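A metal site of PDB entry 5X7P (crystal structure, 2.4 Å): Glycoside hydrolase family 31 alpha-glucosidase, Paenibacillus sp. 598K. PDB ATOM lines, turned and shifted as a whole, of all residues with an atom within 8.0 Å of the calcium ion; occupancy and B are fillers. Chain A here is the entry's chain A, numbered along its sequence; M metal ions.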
ATOM      1  N   THR A 562      17.472   0.320  28.799  1.00  0.00           N
ATOM      2  CA  THR A 562      18.693   1.072  28.848  1.00  0.00           C
ATOM      3  C   THR A 562      19.228   1.175  30.301  1.00  0.00           C
ATOM      4  O   THR A 562      20.400   0.851  30.564  1.00  0.00           O
ATOM      5  CB  THR A 562      18.583   2.457  28.239  1.00  0.00           C
ATOM      6  OG1 THR A 562      18.133   2.329  26.887  1.00  0.00           O
ATOM      7  CG2 THR A 562      19.934   3.153  28.259  1.00  0.00           C
ATOM      8  N   ASP A 666      21.793   9.174  22.888  1.00  0.00           N
ATOM      9  CA  ASP A 666      20.820   8.118  22.596  1.00  0.00           C
ATOM     10  C   ASP A 666      21.024   6.817  23.421  1.00  0.00           C
ATOM     11  O   ASP A 666      20.079   6.225  23.845  1.00  0.00           O
ATOM     12  CB  ASP A 666      20.826   7.809  21.106  1.00  0.00           C
ATOM     13  CG  ASP A 666      19.641   7.059  20.655  1.00  0.00           C
ATOM     14  OD1 ASP A 666      18.568   7.112  21.289  1.00  0.00           O
ATOM     15  OD2 ASP A 666      19.735   6.445  19.619  1.00  0.00           O
ATOM     16  N   ASN A1114      10.897   9.631  14.879  1.00  0.00           N
ATOM     17  CA  ASN A1114      10.512   9.498  16.269  1.00  0.00           C
ATOM     18  C   ASN A1114       9.865   8.111  16.569  1.00  0.00           C
ATOM     19  O   ASN A1114       8.911   7.990  17.366  1.00  0.00           O
ATOM     20  CB  ASN A1114       9.552  10.630  16.674  1.00  0.00           C
ATOM     21  CG  ASN A1114       9.443  10.822  18.190  1.00  0.00           C
ATOM     22  OD1 ASN A1114      10.349  10.451  18.950  1.00  0.00           O
ATOM     23  ND2 ASN A1114       8.330  11.419  18.622  1.00  0.00           N
ATOM     24  N   GLY A1115      10.434   7.072  15.948  1.00  0.00           N
ATOM     25  CA  GLY A1115       9.948   5.711  16.130  1.00  0.00           C
ATOM     26  C   GLY A1115      10.094   5.192  17.547  1.00  0.00           C
ATOM     27  O   GLY A1115       9.338   4.292  17.958  1.00  0.00           O
ATOM     28  N   ASP A1116      11.068   5.775  18.300  1.00  0.00           N
ATOM     29  CA  ASP A1116      11.333   5.406  19.691  1.00  0.00           C
ATOM     30  C   ASP A1116      10.628   6.318  20.720  1.00  0.00           C
ATOM     31  O   ASP A1116      10.787   6.132  21.945  1.00  0.00           O
ATOM     32  CB  ASP A1116      12.836   5.333  19.951  1.00  0.00           C
ATOM     33  CG  ASP A1116      13.583   6.603  19.549  1.00  0.00           C
ATOM     34  OD1 ASP A1116      12.975   7.647  19.226  1.00  0.00           O
ATOM     35  OD2 ASP A1116      14.824   6.552  19.553  1.00  0.00           O
ATOM     36  N   PHE A1117       9.829   7.269  20.209  1.00  0.00           N
ATOM     37  CA  PHE A1117       9.161   8.305  21.010  1.00  0.00           C
ATOM     38  C   PHE A1117      10.086   9.047  22.003  1.00  0.00           C
ATOM     39  O   PHE A1117       9.624   9.577  23.026  1.00  0.00           O
ATOM     40  CB  PHE A1117       7.941   7.695  21.729  1.00  0.00           C
ATOM     41  CG  PHE A1117       7.014   6.920  20.818  1.00  0.00           C
ATOM     42  CD1 PHE A1117       6.115   7.580  19.974  1.00  0.00           C
ATOM     43  CD2 PHE A1117       7.055   5.529  20.781  1.00  0.00           C
ATOM     44  CE1 PHE A1117       5.261   6.873  19.128  1.00  0.00           C
ATOM     45  CE2 PHE A1117       6.195   4.825  19.942  1.00  0.00           C
ATOM     46  CZ  PHE A1117       5.311   5.498  19.106  1.00  0.00           C
ATOM     47  N   GLU A1118      11.391   9.109  21.696  1.00  0.00           N
ATOM     48  CA  GLU A1118      12.326   9.710  22.629  1.00  0.00           C
ATOM     49  C   GLU A1118      12.352  11.207  22.556  1.00  0.00           C
ATOM     50  O   GLU A1118      12.873  11.826  23.465  1.00  0.00           O
ATOM     51  CB  GLU A1118      13.730   9.164  22.420  1.00  0.00           C
ATOM     52  CG  GLU A1118      13.792   7.703  22.835  1.00  0.00           C
ATOM     53  CD  GLU A1118      13.466   7.517  24.286  1.00  0.00           C
ATOM     54  OE1 GLU A1118      13.980   8.222  25.138  1.00  0.00           O
ATOM     55  OE2 GLU A1118      12.691   6.625  24.634  1.00  0.00           O
ATOM     56  N   ARG A1119      11.813  11.776  21.497  1.00  0.00           N
ATOM     57  CA  ARG A1119      11.852  13.207  21.281  1.00  0.00           C
ATOM     58  C   ARG A1119      11.146  13.878  22.436  1.00  0.00           C
ATOM     59  O   ARG A1119      10.118  13.375  22.917  1.00  0.00           O
ATOM     60  CB  ARG A1119      11.133  13.556  19.984  1.00  0.00           C
ATOM     61  CG  ARG A1119      11.191  15.027  19.628  1.00  0.00           C
ATOM     62  CD  ARG A1119      10.853  15.319  18.175  1.00  0.00           C
ATOM     63  NE  ARG A1119      11.660  14.493  17.285  1.00  0.00           N
ATOM     64  CZ  ARG A1119      11.338  14.187  16.034  1.00  0.00           C
ATOM     65  NH1 ARG A1119      10.248  14.643  15.482  1.00  0.00           N
ATOM     66  NH2 ARG A1119      12.126  13.417  15.315  1.00  0.00           N
ATOM     67  N   ILE A1141       2.688  10.289  25.416  1.00  0.00           N
ATOM     68  CA  ILE A1141       4.076   9.834  25.464  1.00  0.00           C
ATOM     69  C   ILE A1141       4.654  10.324  26.784  1.00  0.00           C
ATOM     70  O   ILE A1141       4.547  11.499  27.089  1.00  0.00           O
ATOM     71  CB  ILE A1141       4.917  10.441  24.313  1.00  0.00           C
ATOM     72  CG1 ILE A1141       4.468   9.917  22.940  1.00  0.00           C
ATOM     73  CG2 ILE A1141       6.411  10.128  24.507  1.00  0.00           C
ATOM     74  CD1 ILE A1141       4.948  10.743  21.756  1.00  0.00           C
ATOM     75  N   ASP A1142       5.219   9.430  27.594  1.00  0.00           N
ATOM     76  CA  ASP A1142       5.987   9.805  28.793  1.00  0.00           C
ATOM     77  C   ASP A1142       6.849   8.611  29.263  1.00  0.00           C
ATOM     78  O   ASP A1142       6.985   7.630  28.528  1.00  0.00           O
ATOM     79  CB  ASP A1142       5.076  10.395  29.925  1.00  0.00           C
ATOM     80  CG  ASP A1142       4.106   9.362  30.563  1.00  0.00           C
ATOM     81  OD1 ASP A1142       4.492   8.185  30.786  1.00  0.00           O
ATOM     82  OD2 ASP A1142       2.962   9.782  30.900  1.00  0.00           O
ATOM     83  N   GLY A1152       8.015   1.371  32.924  1.00  0.00           N
ATOM     84  CA  GLY A1152       9.029   2.090  32.146  1.00  0.00           C
ATOM     85  C   GLY A1152       9.002   1.851  30.639  1.00  0.00           C
ATOM     86  O   GLY A1152       8.237   1.028  30.158  1.00  0.00           O
ATOM     87  N   PRO A1153       9.882   2.542  29.893  1.00  0.00           N
ATOM     88  CA  PRO A1153       9.947   2.339  28.455  1.00  0.00           C
ATOM     89  C   PRO A1153      10.641   1.021  28.113  1.00  0.00           C
ATOM     90  O   PRO A1153      11.189   0.374  29.004  1.00  0.00           O
ATOM     91  CB  PRO A1153      10.778   3.557  27.980  1.00  0.00           C
ATOM     92  CG  PRO A1153      11.741   3.730  29.086  1.00  0.00           C
ATOM     93  CD  PRO A1153      10.995   3.370  30.375  1.00  0.00           C
ATOM     94  N   ALA A1154      10.604   0.600  26.855  1.00  0.00           N
ATOM     95  CA  ALA A1154      11.412  -0.543  26.417  1.00  0.00           C
ATOM     96  C   ALA A1154      12.893  -0.175  26.239  1.00  0.00           C
ATOM     97  O   ALA A1154      13.754  -0.995  26.486  1.00  0.00           O
ATOM     98  CB  ALA A1154      10.880  -1.136  25.111  1.00  0.00           C
ATOM     99  N   ARG A1155      13.155   1.032  25.768  1.00  0.00           N
ATOM    100  CA  ARG A1155      14.515   1.534  25.595  1.00  0.00           C
ATOM    101  C   ARG A1155      14.528   3.045  25.855  1.00  0.00           C
ATOM    102  O   ARG A1155      13.599   3.788  25.440  1.00  0.00           O
ATOM    103  CB  ARG A1155      15.075   1.260  24.163  1.00  0.00           C
ATOM    104  CG  ARG A1155      16.619   1.326  24.066  1.00  0.00           C
ATOM    105  CD  ARG A1155      17.178   1.452  22.637  1.00  0.00           C
ATOM    106  NE  ARG A1155      16.801   2.706  21.985  1.00  0.00           N
ATOM    107  CZ  ARG A1155      17.452   3.879  22.097  1.00  0.00           C
ATOM    108  NH1 ARG A1155      18.559   4.011  22.829  1.00  0.00           N
ATOM    109  NH2 ARG A1155      16.969   4.932  21.475  1.00  0.00           N
ATOM    110  N   ARG A1156      15.588   3.469  26.539  1.00  0.00           N
ATOM    111  CA  ARG A1156      15.905   4.865  26.766  1.00  0.00           C
ATOM    112  C   ARG A1156      14.888   5.485  27.721  1.00  0.00           C
ATOM    113  O   ARG A1156      14.717   4.930  28.789  1.00  0.00           O
ATOM    114  CB  ARG A1156      16.106   5.644  25.423  1.00  0.00           C
ATOM    115  CG  ARG A1156      16.854   6.956  25.592  1.00  0.00           C
ATOM    116  CD  ARG A1156      17.167   7.716  24.314  1.00  0.00           C
ATOM    117  NE  ARG A1156      17.920   8.924  24.684  1.00  0.00           N
ATOM    118  CZ  ARG A1156      17.373  10.066  25.102  1.00  0.00           C
ATOM    119  NH1 ARG A1156      16.038  10.226  25.180  1.00  0.00           N
ATOM    120  NH2 ARG A1156      18.184  11.058  25.443  1.00  0.00           N
ATOM    121  N   ASN A1157      14.214   6.574  27.349  1.00  0.00           N
ATOM    122  CA  ASN A1157      13.477   7.374  28.311  1.00  0.00           C
ATOM    123  C   ASN A1157      11.987   7.359  28.183  1.00  0.00           C
ATOM    124  O   ASN A1157      11.329   7.532  29.193  1.00  0.00           O
ATOM    125  CB  ASN A1157      13.891   8.837  28.219  1.00  0.00           C
ATOM    126  CG  ASN A1157      13.785   9.557  29.550  1.00  0.00           C
ATOM    127  OD1 ASN A1157      13.818   8.949  30.625  1.00  0.00           O
ATOM    128  ND2 ASN A1157      13.639  10.858  29.490  1.00  0.00           N
ATOM    129  N   GLN A1158      11.435   7.184  26.982  1.00  0.00           N
ATOM    130  CA  GLN A1158      10.027   7.372  26.774  1.00  0.00           C
ATOM    131  C   GLN A1158       9.351   6.251  26.003  1.00  0.00           C
ATOM    132  O   GLN A1158      10.002   5.503  25.251  1.00  0.00           O
ATOM    133  CB  GLN A1158       9.812   8.722  26.045  1.00  0.00           C
ATOM    134  CG  GLN A1158       9.896   9.879  27.017  1.00  0.00           C
ATOM    135  CD  GLN A1158       9.898  11.249  26.402  1.00  0.00           C
ATOM    136  OE1 GLN A1158       9.724  12.224  27.121  1.00  0.00           O
ATOM    137  NE2 GLN A1158      10.069  11.355  25.098  1.00  0.00           N
ATOM    138  N   ARG A1159       8.038   6.172  26.157  1.00  0.00           N
ATOM    139  CA  ARG A1159       7.217   5.270  25.308  1.00  0.00           C
ATOM    140  C   ARG A1159       5.841   5.885  25.067  1.00  0.00           C
ATOM    141  O   ARG A1159       5.309   6.584  25.917  1.00  0.00           O
ATOM    142  CB  ARG A1159       7.114   3.862  25.933  1.00  0.00           C
ATOM    143  CG  ARG A1159       6.151   3.732  27.116  1.00  0.00           C
ATOM    144  CD  ARG A1159       6.750   4.302  28.394  1.00  0.00           C
ATOM    145  NE  ARG A1159       5.972   4.015  29.597  1.00  0.00           N
ATOM    146  CZ  ARG A1159       4.869   4.637  29.957  1.00  0.00           C
ATOM    147  NH1 ARG A1159       4.364   5.614  29.222  1.00  0.00           N
ATOM    148  NH2 ARG A1159       4.266   4.297  31.086  1.00  0.00           N
ATOM    149  N   ALA A1160       5.259   5.591  23.915  1.00  0.00           N
ATOM    150  CA  ALA A1160       3.873   5.957  23.696  1.00  0.00           C
ATOM    151  C   ALA A1160       3.000   5.111  24.624  1.00  0.00           C
ATOM    152  O   ALA A1160       3.380   3.981  24.990  1.00  0.00           O
ATOM    153  CB  ALA A1160       3.475   5.753  22.238  1.00  0.00           C
ATOM    154  N   TRP A1223       6.886  -6.634  28.150  1.00  0.00           N
ATOM    155  CA  TRP A1223       7.341  -6.170  26.813  1.00  0.00           C
ATOM    156  C   TRP A1223       7.532  -7.328  25.820  1.00  0.00           C
ATOM    157  O   TRP A1223       8.375  -8.199  26.044  1.00  0.00           O
ATOM    158  CB  TRP A1223       8.647  -5.379  26.907  1.00  0.00           C
ATOM    159  CG  TRP A1223       8.508  -3.942  27.357  1.00  0.00           C
ATOM    160  CD1 TRP A1223       9.017  -3.404  28.496  1.00  0.00           C
ATOM    161  CD2 TRP A1223       7.836  -2.841  26.659  1.00  0.00           C
ATOM    162  NE1 TRP A1223       8.728  -2.039  28.563  1.00  0.00           N
ATOM    163  CE2 TRP A1223       7.984  -1.677  27.461  1.00  0.00           C
ATOM    164  CE3 TRP A1223       7.119  -2.746  25.453  1.00  0.00           C
ATOM    165  CZ2 TRP A1223       7.454  -0.417  27.090  1.00  0.00           C
ATOM    166  CZ3 TRP A1223       6.608  -1.495  25.061  1.00  0.00           C
ATOM    167  CH2 TRP A1223       6.757  -0.354  25.887  1.00  0.00           C
ATOM    168  N   ILE A1254       3.665   1.336  23.557  1.00  0.00           N
ATOM    169  CA  ILE A1254       4.313   1.126  22.288  1.00  0.00           C
ATOM    170  C   ILE A1254       5.674   1.768  22.366  1.00  0.00           C
ATOM    171  O   ILE A1254       5.754   2.891  22.817  1.00  0.00           O
ATOM    172  CB  ILE A1254       3.538   1.813  21.138  1.00  0.00           C
ATOM    173  CG1 ILE A1254       2.077   1.361  21.103  1.00  0.00           C
ATOM    174  CG2 ILE A1254       4.212   1.494  19.811  1.00  0.00           C
ATOM    175  CD1 ILE A1254       1.197   2.390  20.433  1.00  0.00           C
ATOM    176  N   ASP A1255       6.707   1.056  21.911  1.00  0.00           N
ATOM    177  CA  ASP A1255       8.067   1.563  21.889  1.00  0.00           C
ATOM    178  C   ASP A1255       8.892   0.962  20.756  1.00  0.00           C
ATOM    179  O   ASP A1255       8.565  -0.105  20.217  1.00  0.00           O
ATOM    180  CB  ASP A1255       8.764   1.283  23.223  1.00  0.00           C
ATOM    181  CG  ASP A1255       9.853   2.293  23.567  1.00  0.00           C
ATOM    182  OD1 ASP A1255      10.010   3.348  22.868  1.00  0.00           O
ATOM    183  OD2 ASP A1255      10.539   2.067  24.576  1.00  0.00           O
ATOM    184  N   GLU A1256       9.978   1.687  20.402  1.00  0.00           N
ATOM    185  CA  GLU A1256      11.057   1.183  19.525  1.00  0.00           C
ATOM    186  C   GLU A1256      10.514   0.689  18.196  1.00  0.00           C
ATOM    187  O   GLU A1256      10.875  -0.398  17.745  1.00  0.00           O
ATOM    188  CB  GLU A1256      11.840   0.044  20.210  1.00  0.00           C
ATOM    189  CG  GLU A1256      12.607   0.465  21.445  1.00  0.00           C
ATOM    190  CD  GLU A1256      13.738   1.424  21.063  1.00  0.00           C
ATOM    191  OE1 GLU A1256      14.759   0.935  20.492  1.00  0.00           O
ATOM    192  OE2 GLU A1256      13.579   2.646  21.318  1.00  0.00           O
ATOM    193  N   VAL A1257       9.676   1.498  17.569  1.00  0.00           N
ATOM    194  CA  VAL A1257       9.121   1.136  16.274  1.00  0.00           C
ATOM    195  C   VAL A1257      10.125   1.408  15.153  1.00  0.00           C
ATOM    196  O   VAL A1257      10.607   2.528  15.066  1.00  0.00           O
ATOM    197  CB  VAL A1257       7.835   1.897  15.996  1.00  0.00           C
ATOM    198  CG1 VAL A1257       7.078   1.242  14.852  1.00  0.00           C
ATOM    199  CG2 VAL A1257       7.000   1.920  17.273  1.00  0.00           C
HETATM  200 CA    CA M   1      11.836   4.677  23.750  1.00  0.00          CA
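The side-chain carboxylate (OE1) of Glu 1118 is in salt-bridge range of the guanidinium group (NH1) of Arg 1156 (2.9 Å).
The backbone NH (N) of Asn 1157 is in hydrogen-bond range of the side-chain carboxylate (OE1) of Glu 1118, at 2.8 Å.
The backbone NH (N) of Glu 1118 sits at hydrogen-bond distance from the side-chain amide oxygen (OD1) of Asn 1114 (3.2 Å).
The side-chain carboxylate (OD2) of Asp 1255 sits at hydrogen-bond distance from the backbone NH (N) of Ala 1154, 2.7 Å away.
The backbone carbonyl oxygen (O) of Phe 1117 is in hydrogen-bond range of the side-chain amide nitrogen (NE2) of Gln 1158 (2.8 Å).
The side-chain amide nitrogen (NE2) of Gln 1158 lies within hydrogen-bond range of the backbone carbonyl oxygen (O) of Arg 1119 (3.0 Å).
NE of Arg 1155 lies within salt-bridge range of OE1 of Glu 1256.
OD1 of Asp 666 is in salt-bridge range of NH2 of Arg 1155 (2.7 Å).
Glu 1256 touches the calcium ion.
Six residues have an atom within 4 Å of the calcium ion: Asp 1116, Glu 1118, Arg 1155, Gln 1158, Asp 1255 and Glu 1256.
The nearest printed residue that does not touch the calcium ion is Pro 1153 (4.5 Å).
The calcium ion is bound by OE2 of Glu 1118 (2.3 Å), OD1 of Asp 1255 (2.4 Å), O of Gln 1158 (2.5 Å), O of Asp 1116 (2.5 Å) and O of Arg 1155 (2.6 Å).
Slightly farther from the calcium ion lies OD2 of Asp 1255 (3.0 Å).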
